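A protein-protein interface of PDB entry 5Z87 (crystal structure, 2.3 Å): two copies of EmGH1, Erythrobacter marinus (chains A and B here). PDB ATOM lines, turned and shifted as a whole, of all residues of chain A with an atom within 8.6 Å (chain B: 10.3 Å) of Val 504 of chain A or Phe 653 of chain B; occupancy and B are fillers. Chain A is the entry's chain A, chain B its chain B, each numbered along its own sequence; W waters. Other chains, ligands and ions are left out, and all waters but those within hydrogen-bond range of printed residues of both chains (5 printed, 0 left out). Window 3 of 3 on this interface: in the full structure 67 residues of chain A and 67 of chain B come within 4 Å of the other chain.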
ATOM      1  N   ALA A 484      31.920  19.114 -24.893  1.00  0.00           N
ATOM      2  CA  ALA A 484      30.690  18.742 -24.213  1.00  0.00           C
ATOM      3  C   ALA A 484      29.694  19.891 -24.304  1.00  0.00           C
ATOM      4  O   ALA A 484      30.077  21.064 -24.294  1.00  0.00           O
ATOM      5  CB  ALA A 484      30.948  18.393 -22.740  1.00  0.00           C
ATOM      6  N   ILE A 485      28.409  19.541 -24.403  1.00  0.00           N
ATOM      7  CA  ILE A 485      27.329  20.524 -24.349  1.00  0.00           C
ATOM      8  C   ILE A 485      26.957  20.741 -22.888  1.00  0.00           C
ATOM      9  O   ILE A 485      27.031  21.859 -22.359  1.00  0.00           O
ATOM     10  CB  ILE A 485      26.118  20.065 -25.183  1.00  0.00           C
ATOM     11  CG1 ILE A 485      26.469  20.077 -26.675  1.00  0.00           C
ATOM     12  CG2 ILE A 485      24.892  20.923 -24.881  1.00  0.00           C
ATOM     13  CD1 ILE A 485      25.442  19.406 -27.563  1.00  0.00           C
ATOM     14  N   THR A 486      26.585  19.661 -22.219  1.00  0.00           N
ATOM     15  CA  THR A 486      26.249  19.697 -20.807  1.00  0.00           C
ATOM     16  C   THR A 486      27.298  18.928 -20.016  1.00  0.00           C
ATOM     17  O   THR A 486      27.858  17.939 -20.496  1.00  0.00           O
ATOM     18  CB  THR A 486      24.854  19.118 -20.579  1.00  0.00           C
ATOM     19  OG1 THR A 486      24.646  18.019 -21.478  1.00  0.00           O
ATOM     20  CG2 THR A 486      23.815  20.190 -20.866  1.00  0.00           C
ATOM     21  N   ALA A 487      27.584  19.409 -18.809  1.00  0.00           N
ATOM     22  CA  ALA A 487      28.635  18.803 -18.003  1.00  0.00           C
ATOM     23  C   ALA A 487      28.185  17.447 -17.475  1.00  0.00           C
ATOM     24  O   ALA A 487      27.033  17.267 -17.070  1.00  0.00           O
ATOM     25  CB  ALA A 487      29.026  19.722 -16.853  1.00  0.00           C
ATOM     26  N   GLY A 488      29.106  16.485 -17.500  1.00  0.00           N
ATOM     27  CA  GLY A 488      28.795  15.122 -17.140  1.00  0.00           C
ATOM     28  C   GLY A 488      28.156  14.307 -18.241  1.00  0.00           C
ATOM     29  O   GLY A 488      27.880  13.118 -18.029  1.00  0.00           O
ATOM     30  N   ASP A 489      27.904  14.902 -19.403  1.00  0.00           N
ATOM     31  CA  ASP A 489      27.340  14.188 -20.545  1.00  0.00           C
ATOM     32  C   ASP A 489      28.428  14.108 -21.615  1.00  0.00           C
ATOM     33  O   ASP A 489      28.438  14.861 -22.592  1.00  0.00           O
ATOM     34  CB  ASP A 489      26.032  14.872 -21.058  1.00  0.00           C
ATOM     35  CG  ASP A 489      24.899  14.825 -20.020  1.00  0.00           C
ATOM     36  OD1 ASP A 489      24.655  13.740 -19.435  1.00  0.00           O
ATOM     37  OD2 ASP A 489      24.255  15.876 -19.787  1.00  0.00           O
ATOM     38  N   ASP A 501      19.591  15.327 -10.871  1.00  0.00           N
ATOM     39  CA  ASP A 501      20.721  16.241 -10.983  1.00  0.00           C
ATOM     40  C   ASP A 501      20.377  17.267 -12.056  1.00  0.00           C
ATOM     41  O   ASP A 501      20.316  16.934 -13.244  1.00  0.00           O
ATOM     42  CB  ASP A 501      22.006  15.491 -11.329  1.00  0.00           C
ATOM     43  CG  ASP A 501      22.661  14.859 -10.115  1.00  0.00           C
ATOM     44  OD1 ASP A 501      22.054  13.944  -9.518  1.00  0.00           O
ATOM     45  OD2 ASP A 501      23.785  15.276  -9.758  1.00  0.00           O
ATOM     46  N   GLU A 502      20.124  18.504 -11.636  1.00  0.00           N
ATOM     47  CA  GLU A 502      19.833  19.560 -12.592  1.00  0.00           C
ATOM     48  C   GLU A 502      21.000  19.715 -13.554  1.00  0.00           C
ATOM     49  O   GLU A 502      22.167  19.641 -13.160  1.00  0.00           O
ATOM     50  CB  GLU A 502      19.561  20.877 -11.873  1.00  0.00           C
ATOM     51  CG  GLU A 502      18.246  20.909 -11.125  1.00  0.00           C
ATOM     52  CD  GLU A 502      18.367  21.612  -9.790  1.00  0.00           C
ATOM     53  OE1 GLU A 502      19.265  22.471  -9.653  1.00  0.00           O
ATOM     54  OE2 GLU A 502      17.568  21.307  -8.876  1.00  0.00           O
ATOM     55  N   SER A 503      20.679  19.919 -14.823  1.00  0.00           N
ATOM     56  CA  SER A 503      21.709  19.985 -15.844  1.00  0.00           C
ATOM     57  C   SER A 503      22.474  21.301 -15.742  1.00  0.00           C
ATOM     58  O   SER A 503      21.892  22.362 -15.485  1.00  0.00           O
ATOM     59  CB  SER A 503      21.067  19.828 -17.221  1.00  0.00           C
ATOM     60  OG  SER A 503      21.997  20.035 -18.260  1.00  0.00           O
ATOM     61  N   VAL A 504      23.795  21.224 -15.917  1.00  0.00           N
ATOM     62  CA  VAL A 504      24.667  22.395 -15.931  1.00  0.00           C
ATOM     63  C   VAL A 504      25.423  22.438 -17.259  1.00  0.00           C
ATOM     64  O   VAL A 504      25.727  21.404 -17.859  1.00  0.00           O
ATOM     65  CB  VAL A 504      25.645  22.402 -14.731  1.00  0.00           C
ATOM     66  CG1 VAL A 504      24.914  22.032 -13.456  1.00  0.00           C
ATOM     67  CG2 VAL A 504      26.766  21.435 -14.950  1.00  0.00           C
ATOM     68  N   GLN A 505      25.708  23.648 -17.734  1.00  0.00           N
ATOM     69  CA  GLN A 505      26.391  23.782 -19.012  1.00  0.00           C
ATOM     70  C   GLN A 505      27.851  23.347 -18.895  1.00  0.00           C
ATOM     71  O   GLN A 505      28.482  23.493 -17.848  1.00  0.00           O
ATOM     72  CB  GLN A 505      26.303  25.222 -19.512  1.00  0.00           C
ATOM     73  CG  GLN A 505      26.654  25.376 -20.980  1.00  0.00           C
ATOM     74  CD  GLN A 505      26.482  26.801 -21.464  1.00  0.00           C
ATOM     75  OE1 GLN A 505      25.915  27.631 -20.762  1.00  0.00           O
ATOM     76  NE2 GLN A 505      26.974  27.092 -22.666  1.00  0.00           N
ATOM     77  N   ALA A 506      28.388  22.807 -19.981  1.00  0.00           N
ATOM     78  CA  ALA A 506      29.752  22.301 -19.948  1.00  0.00           C
ATOM     79  C   ALA A 506      30.750  23.435 -19.754  1.00  0.00           C
ATOM     80  O   ALA A 506      30.517  24.578 -20.162  1.00  0.00           O
ATOM     81  CB  ALA A 506      30.074  21.538 -21.228  1.00  0.00           C
ATOM     82  N   ASP A 507      31.876  23.105 -19.113  1.00  0.00           N
ATOM     83  CA  ASP A 507      32.875  24.119 -18.783  1.00  0.00           C
ATOM     84  C   ASP A 507      33.648  24.538 -20.033  1.00  0.00           C
ATOM     85  O   ASP A 507      34.169  23.677 -20.753  1.00  0.00           O
ATOM     86  CB  ASP A 507      33.832  23.600 -17.712  1.00  0.00           C
ATOM     87  CG  ASP A 507      34.970  24.562 -17.439  1.00  0.00           C
ATOM     88  OD1 ASP A 507      34.717  25.778 -17.326  1.00  0.00           O
ATOM     89  OD2 ASP A 507      36.127  24.105 -17.347  1.00  0.00           O
ATOM     90  N   ASN A 535      21.029  18.767 -27.049  1.00  0.00           N
ATOM     91  CA  ASN A 535      20.613  17.499 -26.458  1.00  0.00           C
ATOM     92  C   ASN A 535      19.322  17.716 -25.677  1.00  0.00           C
ATOM     93  O   ASN A 535      18.723  18.801 -25.693  1.00  0.00           O
ATOM     94  CB  ASN A 535      21.731  16.878 -25.599  1.00  0.00           C
ATOM     95  CG  ASN A 535      22.143  17.755 -24.433  1.00  0.00           C
ATOM     96  OD1 ASN A 535      21.351  18.543 -23.914  1.00  0.00           O
ATOM     97  ND2 ASN A 535      23.394  17.616 -24.008  1.00  0.00           N
ATOM     98  N   GLU A 536      18.914  16.658 -24.982  1.00  0.00           N
ATOM     99  CA  GLU A 536      17.670  16.603 -24.233  1.00  0.00           C
ATOM    100  C   GLU A 536      17.698  17.483 -22.997  1.00  0.00           C
ATOM    101  O   GLU A 536      16.668  17.613 -22.334  1.00  0.00           O
ATOM    102  CB  GLU A 536      17.373  15.142 -23.865  1.00  0.00           C
ATOM    103  CG  GLU A 536      17.020  14.258 -25.078  1.00  0.00           C
ATOM    104  CD  GLU A 536      18.235  13.728 -25.860  1.00  0.00           C
ATOM    105  OE1 GLU A 536      18.016  12.946 -26.817  1.00  0.00           O
ATOM    106  OE2 GLU A 536      19.397  14.087 -25.536  1.00  0.00           O
ATOM    107  N   SER A 537      18.837  18.102 -22.682  1.00  0.00           N
ATOM    108  CA  SER A 537      18.886  19.137 -21.658  1.00  0.00           C
ATOM    109  C   SER A 537      18.793  20.557 -22.224  1.00  0.00           C
ATOM    110  O   SER A 537      18.335  21.457 -21.516  1.00  0.00           O
ATOM    111  CB  SER A 537      20.172  19.015 -20.831  1.00  0.00           C
ATOM    112  OG  SER A 537      20.055  18.005 -19.857  1.00  0.00           O
ATOM    113  N   THR A 538      19.204  20.797 -23.474  1.00  0.00           N
ATOM    114  CA  THR A 538      19.134  22.160 -24.002  1.00  0.00           C
ATOM    115  C   THR A 538      17.812  22.456 -24.706  1.00  0.00           C
ATOM    116  O   THR A 538      17.419  23.627 -24.785  1.00  0.00           O
ATOM    117  CB  THR A 538      20.321  22.446 -24.932  1.00  0.00           C
ATOM    118  OG1 THR A 538      20.342  21.534 -26.034  1.00  0.00           O
ATOM    119  CG2 THR A 538      21.635  22.308 -24.149  1.00  0.00           C
ATOM    120  N   ALA A 539      17.120  21.431 -25.199  1.00  0.00           N
ATOM    121  CA  ALA A 539      15.720  21.516 -25.603  1.00  0.00           C
ATOM    122  C   ALA A 539      14.961  20.507 -24.752  1.00  0.00           C
ATOM    123  O   ALA A 539      15.185  19.295 -24.871  1.00  0.00           O
ATOM    124  CB  ALA A 539      15.535  21.225 -27.094  1.00  0.00           C
ATOM    125  N   ARG A 540      14.102  20.996 -23.868  1.00  0.00           N
ATOM    126  CA  ARG A 540      13.273  20.090 -23.092  1.00  0.00           C
ATOM    127  C   ARG A 540      12.042  20.840 -22.617  1.00  0.00           C
ATOM    128  O   ARG A 540      11.959  22.070 -22.681  1.00  0.00           O
ATOM    129  CB  ARG A 540      14.035  19.489 -21.906  1.00  0.00           C
ATOM    130  CG  ARG A 540      14.263  20.450 -20.751  1.00  0.00           C
ATOM    131  CD  ARG A 540      14.832  19.734 -19.535  1.00  0.00           C
ATOM    132  NE  ARG A 540      14.078  18.527 -19.180  1.00  0.00           N
ATOM    133  CZ  ARG A 540      14.614  17.312 -19.091  1.00  0.00           C
ATOM    134  NH1 ARG A 540      15.911  17.139 -19.329  1.00  0.00           N
ATOM    135  NH2 ARG A 540      13.861  16.271 -18.756  1.00  0.00           N
ATOM    136  N   ASP A 547      12.375  25.736 -10.772  1.00  0.00           N
ATOM    137  CA  ASP A 547      12.835  26.621 -11.839  1.00  0.00           C
ATOM    138  C   ASP A 547      13.287  25.786 -13.031  1.00  0.00           C
ATOM    139  O   ASP A 547      14.382  25.986 -13.561  1.00  0.00           O
ATOM    140  CB  ASP A 547      13.971  27.521 -11.331  1.00  0.00           C
ATOM    141  CG  ASP A 547      14.363  28.614 -12.329  1.00  0.00           C
ATOM    142  OD1 ASP A 547      13.511  29.059 -13.129  1.00  0.00           O
ATOM    143  OD2 ASP A 547      15.539  29.021 -12.310  1.00  0.00           O
ATOM    144  N   ARG A 549      13.881  24.503 -16.661  1.00  0.00           N
ATOM    145  CA  ARG A 549      14.150  25.311 -17.848  1.00  0.00           C
ATOM    146  C   ARG A 549      14.400  24.435 -19.062  1.00  0.00           C
ATOM    147  O   ARG A 549      14.994  23.358 -18.951  1.00  0.00           O
ATOM    148  CB  ARG A 549      15.355  26.237 -17.646  1.00  0.00           C
ATOM    149  CG  ARG A 549      15.184  27.224 -16.513  1.00  0.00           C
ATOM    150  CD  ARG A 549      16.277  28.213 -16.519  1.00  0.00           C
ATOM    151  NE  ARG A 549      16.286  28.996 -15.301  1.00  0.00           N
ATOM    152  CZ  ARG A 549      16.815  30.213 -15.214  1.00  0.00           C
ATOM    153  NH1 ARG A 549      16.791  30.873 -14.064  1.00  0.00           N
ATOM    154  NH2 ARG A 549      17.367  30.767 -16.285  1.00  0.00           N
ATOM    155  N   GLY A 550      13.964  24.913 -20.224  1.00  0.00           N
ATOM    156  CA  GLY A 550      14.042  24.126 -21.437  1.00  0.00           C
ATOM    157  C   GLY A 550      13.946  24.932 -22.711  1.00  0.00           C
ATOM    158  O   GLY A 550      14.237  24.425 -23.795  1.00  0.00           O
ATOM    159  N   ASP A 551      13.529  26.183 -22.595  1.00  0.00           N
ATOM    160  CA  ASP A 551      13.421  27.082 -23.732  1.00  0.00           C
ATOM    161  C   ASP A 551      14.713  27.891 -23.853  1.00  0.00           C
ATOM    162  O   ASP A 551      15.388  28.142 -22.855  1.00  0.00           O
ATOM    163  CB  ASP A 551      12.192  27.990 -23.550  1.00  0.00           C
ATOM    164  CG  ASP A 551      10.936  27.204 -23.052  1.00  0.00           C
ATOM    165  OD1 ASP A 551      10.560  26.191 -23.686  1.00  0.00           O
ATOM    166  OD2 ASP A 551      10.324  27.590 -22.029  1.00  0.00           O
ATOM    167  N   ARG A 552      15.068  28.280 -25.082  1.00  0.00           N
ATOM    168  CA  ARG A 552      16.310  29.012 -25.340  1.00  0.00           C
ATOM    169  C   ARG A 552      16.022  30.398 -25.912  1.00  0.00           C
ATOM    170  O   ARG A 552      15.065  30.596 -26.667  1.00  0.00           O
ATOM    171  CB  ARG A 552      17.248  28.248 -26.318  1.00  0.00           C
ATOM    172  CG  ARG A 552      17.918  27.017 -25.728  1.00  0.00           C
ATOM    173  CD  ARG A 552      19.006  26.410 -26.636  1.00  0.00           C
ATOM    174  NE  ARG A 552      20.059  27.368 -26.971  1.00  0.00           N
ATOM    175  CZ  ARG A 552      20.783  27.326 -28.092  1.00  0.00           C
ATOM    176  NH1 ARG A 552      20.587  26.361 -28.988  1.00  0.00           N
ATOM    177  NH2 ARG A 552      21.704  28.256 -28.319  1.00  0.00           N
ATOM    178  N   ASP A 553      16.874  31.359 -25.561  1.00  0.00           N
ATOM    179  CA  ASP A 553      16.800  32.703 -26.126  1.00  0.00           C
ATOM    180  C   ASP A 553      17.826  32.905 -27.234  1.00  0.00           C
ATOM    181  O   ASP A 553      18.267  34.029 -27.481  1.00  0.00           O
ATOM    182  CB  ASP A 553      16.977  33.754 -25.032  1.00  0.00           C
ATOM    183  CG  ASP A 553      18.258  33.556 -24.254  1.00  0.00           C
ATOM    184  OD1 ASP A 553      19.014  32.628 -24.620  1.00  0.00           O
ATOM    185  OD2 ASP A 553      18.510  34.317 -23.290  1.00  0.00           O
ATOM    186  N   ILE A 558      24.851  25.759 -29.146  1.00  0.00           N
ATOM    187  CA  ILE A 558      25.172  26.263 -27.818  1.00  0.00           C
ATOM    188  C   ILE A 558      26.635  25.980 -27.501  1.00  0.00           C
ATOM    189  O   ILE A 558      27.218  24.988 -27.961  1.00  0.00           O
ATOM    190  CB  ILE A 558      24.225  25.649 -26.768  1.00  0.00           C
ATOM    191  CG1 ILE A 558      24.361  26.380 -25.442  1.00  0.00           C
ATOM    192  CG2 ILE A 558      24.499  24.158 -26.572  1.00  0.00           C
ATOM    193  CD1 ILE A 558      23.194  26.108 -24.521  1.00  0.00           C
ATOM    194  N   GLY A 559      27.242  26.895 -26.745  1.00  0.00           N
ATOM    195  CA  GLY A 559      28.533  26.627 -26.126  1.00  0.00           C
ATOM    196  C   GLY A 559      29.697  26.734 -27.098  1.00  0.00           C
ATOM    197  O   GLY A 559      29.810  27.695 -27.872  1.00  0.00           O
ATOM    198  N   ARG B 631      17.672  41.537 -21.579  1.00  0.00           N
ATOM    199  CA  ARG B 631      19.110  41.280 -21.711  1.00  0.00           C
ATOM    200  C   ARG B 631      19.516  41.035 -23.158  1.00  0.00           C
ATOM    201  O   ARG B 631      20.597  41.464 -23.585  1.00  0.00           O
ATOM    202  CB  ARG B 631      19.516  40.091 -20.837  1.00  0.00           C
ATOM    203  CG  ARG B 631      19.551  40.477 -19.386  1.00  0.00           C
ATOM    204  CD  ARG B 631      19.826  39.358 -18.400  1.00  0.00           C
ATOM    205  NE  ARG B 631      19.662  39.935 -17.075  1.00  0.00           N
ATOM    206  CZ  ARG B 631      20.621  40.584 -16.419  1.00  0.00           C
ATOM    207  NH1 ARG B 631      21.840  40.672 -16.942  1.00  0.00           N
ATOM    208  NH2 ARG B 631      20.368  41.126 -15.234  1.00  0.00           N
ATOM    209  N   ASN B 632      18.680  40.328 -23.918  1.00  0.00           N
ATOM    210  CA  ASN B 632      18.945  40.101 -25.325  1.00  0.00           C
ATOM    211  C   ASN B 632      17.619  39.914 -26.044  1.00  0.00           C
ATOM    212  O   ASN B 632      16.588  39.630 -25.427  1.00  0.00           O
ATOM    213  CB  ASN B 632      19.855  38.881 -25.556  1.00  0.00           C
ATOM    214  CG  ASN B 632      19.209  37.558 -25.126  1.00  0.00           C
ATOM    215  OD1 ASN B 632      18.324  37.029 -25.809  1.00  0.00           O
ATOM    216  ND2 ASN B 632      19.684  37.001 -24.015  1.00  0.00           N
ATOM    217  N   GLN B 635      14.807  37.110 -25.781  1.00  0.00           N
ATOM    218  CA  GLN B 635      13.969  37.037 -24.592  1.00  0.00           C
ATOM    219  C   GLN B 635      12.696  37.870 -24.722  1.00  0.00           C
ATOM    220  O   GLN B 635      11.968  38.022 -23.735  1.00  0.00           O
ATOM    221  CB  GLN B 635      14.761  37.479 -23.358  1.00  0.00           C
ATOM    222  CG  GLN B 635      16.054  36.697 -23.126  1.00  0.00           C
ATOM    223  CD  GLN B 635      16.660  36.960 -21.739  1.00  0.00           C
ATOM    224  OE1 GLN B 635      16.393  37.989 -21.121  1.00  0.00           O
ATOM    225  NE2 GLN B 635      17.488  36.029 -21.259  1.00  0.00           N
ATOM    226  N   ARG B 649       8.346  30.623 -16.830  1.00  0.00           N
ATOM    227  CA  ARG B 649       9.536  29.812 -17.060  1.00  0.00           C
ATOM    228  C   ARG B 649      10.662  30.654 -17.666  1.00  0.00           C
ATOM    229  O   ARG B 649      10.416  31.576 -18.454  1.00  0.00           O
ATOM    230  CB  ARG B 649       9.209  28.630 -17.976  1.00  0.00           C
ATOM    231  CG  ARG B 649       8.067  27.711 -17.452  1.00  0.00           C
ATOM    232  CD  ARG B 649       8.472  26.898 -16.204  1.00  0.00           C
ATOM    233  NE  ARG B 649       8.597  27.728 -15.004  1.00  0.00           N
ATOM    234  CZ  ARG B 649       8.989  27.271 -13.822  1.00  0.00           C
ATOM    235  NH1 ARG B 649       9.085  28.104 -12.796  1.00  0.00           N
ATOM    236  NH2 ARG B 649       9.282  25.975 -13.665  1.00  0.00           N
ATOM    237  N   ASN B 650      11.893  30.325 -17.293  1.00  0.00           N
ATOM    238  CA  ASN B 650      13.090  31.059 -17.683  1.00  0.00           C
ATOM    239  C   ASN B 650      13.873  30.293 -18.753  1.00  0.00           C
ATOM    240  O   ASN B 650      13.642  29.104 -18.999  1.00  0.00           O
ATOM    241  CB  ASN B 650      13.961  31.321 -16.450  1.00  0.00           C
ATOM    242  CG  ASN B 650      13.263  32.190 -15.412  1.00  0.00           C
ATOM    243  OD1 ASN B 650      12.794  33.270 -15.730  1.00  0.00           O
ATOM    244  ND2 ASN B 650      13.217  31.729 -14.163  1.00  0.00           N
ATOM    245  N   TYR B 651      14.806  30.988 -19.401  1.00  0.00           N
ATOM    246  CA  TYR B 651      15.538  30.367 -20.501  1.00  0.00           C
ATOM    247  C   TYR B 651      16.711  29.541 -19.982  1.00  0.00           C
ATOM    248  O   TYR B 651      17.338  29.869 -18.971  1.00  0.00           O
ATOM    249  CB  TYR B 651      16.029  31.415 -21.490  1.00  0.00           C
ATOM    250  CG  TYR B 651      14.911  32.177 -22.167  1.00  0.00           C
ATOM    251  CD1 TYR B 651      14.246  31.647 -23.268  1.00  0.00           C
ATOM    252  CD2 TYR B 651      14.531  33.434 -21.703  1.00  0.00           C
ATOM    253  CE1 TYR B 651      13.224  32.351 -23.893  1.00  0.00           C
ATOM    254  CE2 TYR B 651      13.524  34.146 -22.310  1.00  0.00           C
ATOM    255  CZ  TYR B 651      12.867  33.601 -23.403  1.00  0.00           C
ATOM    256  OH  TYR B 651      11.872  34.328 -23.997  1.00  0.00           O
ATOM    257  N   VAL B 652      17.008  28.452 -20.691  1.00  0.00           N
ATOM    258  CA  VAL B 652      17.996  27.500 -20.197  1.00  0.00           C
ATOM    259  C   VAL B 652      19.383  28.126 -20.289  1.00  0.00           C
ATOM    260  O   VAL B 652      19.731  28.757 -21.296  1.00  0.00           O
ATOM    261  CB  VAL B 652      17.890  26.171 -20.965  1.00  0.00           C
ATOM    262  CG1 VAL B 652      17.971  26.405 -22.423  1.00  0.00           C
ATOM    263  CG2 VAL B 652      18.982  25.203 -20.550  1.00  0.00           C
ATOM    264  N   PHE B 653      20.153  28.015 -19.198  1.00  0.00           N
ATOM    265  CA  PHE B 653      21.539  28.494 -19.122  1.00  0.00           C
ATOM    266  C   PHE B 653      21.653  29.998 -19.398  1.00  0.00           C
ATOM    267  O   PHE B 653      22.638  30.470 -19.969  1.00  0.00           O
ATOM    268  CB  PHE B 653      22.449  27.697 -20.072  1.00  0.00           C
ATOM    269  CG  PHE B 653      22.447  26.201 -19.811  1.00  0.00           C
ATOM    270  CD1 PHE B 653      22.275  25.708 -18.530  1.00  0.00           C
ATOM    271  CD2 PHE B 653      22.624  25.298 -20.847  1.00  0.00           C
ATOM    272  CE1 PHE B 653      22.263  24.339 -18.280  1.00  0.00           C
ATOM    273  CE2 PHE B 653      22.622  23.932 -20.609  1.00  0.00           C
ATOM    274  CZ  PHE B 653      22.439  23.453 -19.323  1.00  0.00           C
ATOM    275  N   SER B 654      20.658  30.785 -19.007  1.00  0.00           N
ATOM    276  CA  SER B 654      20.671  32.189 -19.391  1.00  0.00           C
ATOM    277  C   SER B 654      19.930  33.009 -18.350  1.00  0.00           C
ATOM    278  O   SER B 654      18.757  32.737 -18.066  1.00  0.00           O
ATOM    279  CB  SER B 654      20.049  32.369 -20.774  1.00  0.00           C
ATOM    280  OG  SER B 654      20.080  33.732 -21.168  1.00  0.00           O
ATOM    281  N   ASP B 655      20.613  34.003 -17.780  1.00  0.00           N
ATOM    282  CA  ASP B 655      19.945  34.966 -16.913  1.00  0.00           C
ATOM    283  C   ASP B 655      18.746  35.560 -17.650  1.00  0.00           C
ATOM    284  O   ASP B 655      18.902  36.187 -18.702  1.00  0.00           O
ATOM    285  CB  ASP B 655      20.933  36.062 -16.496  1.00  0.00           C
ATOM    286  CG  ASP B 655      20.380  36.974 -15.413  1.00  0.00           C
ATOM    287  OD1 ASP B 655      19.169  36.887 -15.089  1.00  0.00           O
ATOM    288  OD2 ASP B 655      21.170  37.779 -14.872  1.00  0.00           O
ATOM    289  N   SER B 656      17.544  35.322 -17.120  1.00  0.00           N
ATOM    290  CA  SER B 656      16.319  35.731 -17.784  1.00  0.00           C
ATOM    291  C   SER B 656      15.677  36.945 -17.141  1.00  0.00           C
ATOM    292  O   SER B 656      14.628  37.390 -17.614  1.00  0.00           O
ATOM    293  CB  SER B 656      15.304  34.576 -17.820  1.00  0.00           C
ATOM    294  OG  SER B 656      15.889  33.394 -18.327  1.00  0.00           O
ATOM    295  N   THR B 657      16.262  37.471 -16.067  1.00  0.00           N
ATOM    296  CA  THR B 657      15.814  38.725 -15.491  1.00  0.00           C
ATOM    297  C   THR B 657      16.036  39.864 -16.485  1.00  0.00           C
ATOM    298  O   THR B 657      16.841  39.746 -17.410  1.00  0.00           O
ATOM    299  CB  THR B 657      16.573  39.024 -14.197  1.00  0.00           C
ATOM    300  OG1 THR B 657      17.953  39.248 -14.506  1.00  0.00           O
ATOM    301  CG2 THR B 657      16.442  37.871 -13.200  1.00  0.00           C
HETATM  302  O   HOH W   1      12.185  27.233 -20.237  1.00  0.00           O
HETATM  303  O   HOH W   2      11.241  30.225 -11.365  1.00  0.00           O
HETATM  304  O   HOH W   3      18.900  30.058 -23.514  1.00  0.00           O
HETATM  305  O   HOH W   4      17.148  33.806 -14.525  1.00  0.00           O
HETATM  306  O   HOH W   5      11.829  28.331 -15.303  1.00  0.00           O
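The side-chain carboxylate (OD2) of Asp 553 of chain A sits at hydrogen-bond distance from the side-chain amide nitrogen (NE2) of Gln 635 of chain B (2.8 Å).
The side-chain amide nitrogen of Asn 632 of chain B is in hydrogen-bond range of the side-chain carboxylate of Asp 553 of chain A (3.0 Å).
ND2 of Asn 650 of chain B sits at hydrogen-bond distance from OD1 of Asp 547 of chain A, 2.9 Å away.
The side-chain carboxylate (OD2) of Asp 553 of chain A lies within hydrogen-bond range of the side-chain hydroxyl (OG) of Ser 654 of chain B (2.7 Å).
The guanidinium group (NH2) of Arg 549 of chain A sits at hydrogen-bond distance from the backbone carbonyl oxygen (O) of Ser 654 of chain B (3.0 Å).
The guanidinium group of Arg 549 of chain A lies within hydrogen-bond range of the backbone carbonyl oxygen of Tyr 651 of chain B.
O of Asp 551 of chain A lies within hydrogen-bond range of N of Val 652 of chain B.
OG1 of Thr 538 of chain A lies within hydrogen-bond range of N of Asn 535 of chain A (3.0 Å).
ND2 of Asn 535 of chain A sits at hydrogen-bond distance from OG1 of Thr 486 of chain A, 2.9 Å away.
The backbone NH of Tyr 651 of chain B lies within hydrogen-bond range of the side-chain hydroxyl of Ser 656 of chain B.
Phe 653 of chain B touches Ser 503 of chain A.
Phe 653 of chain B touches Val 504 of chain A.
CB of Phe 653 of chain B touches OE1 of Gln 505 of chain A (3.5 Å).
Arg 549 of chain A touches Val 652 of chain B.
Ser 656 of chain B touches Arg 549 of chain A.
Arg 552 of chain A touches Tyr 651 of chain B (C to CD1, 3.4 Å).
Tyr 651 of chain B touches Asp 553 of chain A (CD1 to N, 3.5 Å).
Val 504 of chain A touches just one residue of chain B: Phe 653.
Gln 505 of chain A touches just one residue of chain B: Phe 653 (3.5 Å).
No residue of chain B comes within 4 Å of Ala 506 of chain A.
Ser 654 of chain B touches just these residues of chain A: Arg 549 and Asp 553.
Of the printed residues of chain A, Asn 632 of chain B touches Asp 553.
Of the printed residues of chain A, Gln 635 of chain B touches Asp 553.
Printed residues of chain B within 4 Å of Arg 549 of chain A: Asn 650, Tyr 651, Val 652, Ser 654 and Ser 656.
Printed residues of chain B within 4 Å of Arg 552 of chain A: Tyr 651 (3.4 Å) and Val 652 (3.4 Å).
The nearest residue of chain B that does not touch Val 504 of chain A is Val 652 of chain B (7.7 Å).
Printed residues of chain B that touch a printed residue of chain A: Asn 632, Gln 635, Asn 650, Tyr 651, Val 652, Phe 653, Ser 654 and Ser 656.
Of the 27 printed residues of chain A, 12 touch a printed residue of chain B.
Hydrophobic or aromatic side chains of chain A within 4 Å of the printed part of chain B: Ile 558.
Among the printed residues, no Asp or Glu carboxylate lies within 4 Å of a Lys or Arg side-chain nitrogen of the other chain.
No position is printed for both chains.
Of the 21 pairs that touch across the chains among the printed residues, none has its exchanged pair printed and touching as well.
Water W1 lies within hydrogen-bond range of OD2 of Asp 551 of chain A (2.6 Å), O of Asn 650 of chain B (2.7 Å) and N of Gly 550 of chain A (2.9 Å).
Water W5 lies within hydrogen-bond range of N of Asn 650 of chain B (2.8 Å), OD1 of Asp 547 of chain A (2.8 Å) and NE of Arg 649 of chain B (3.3 Å).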
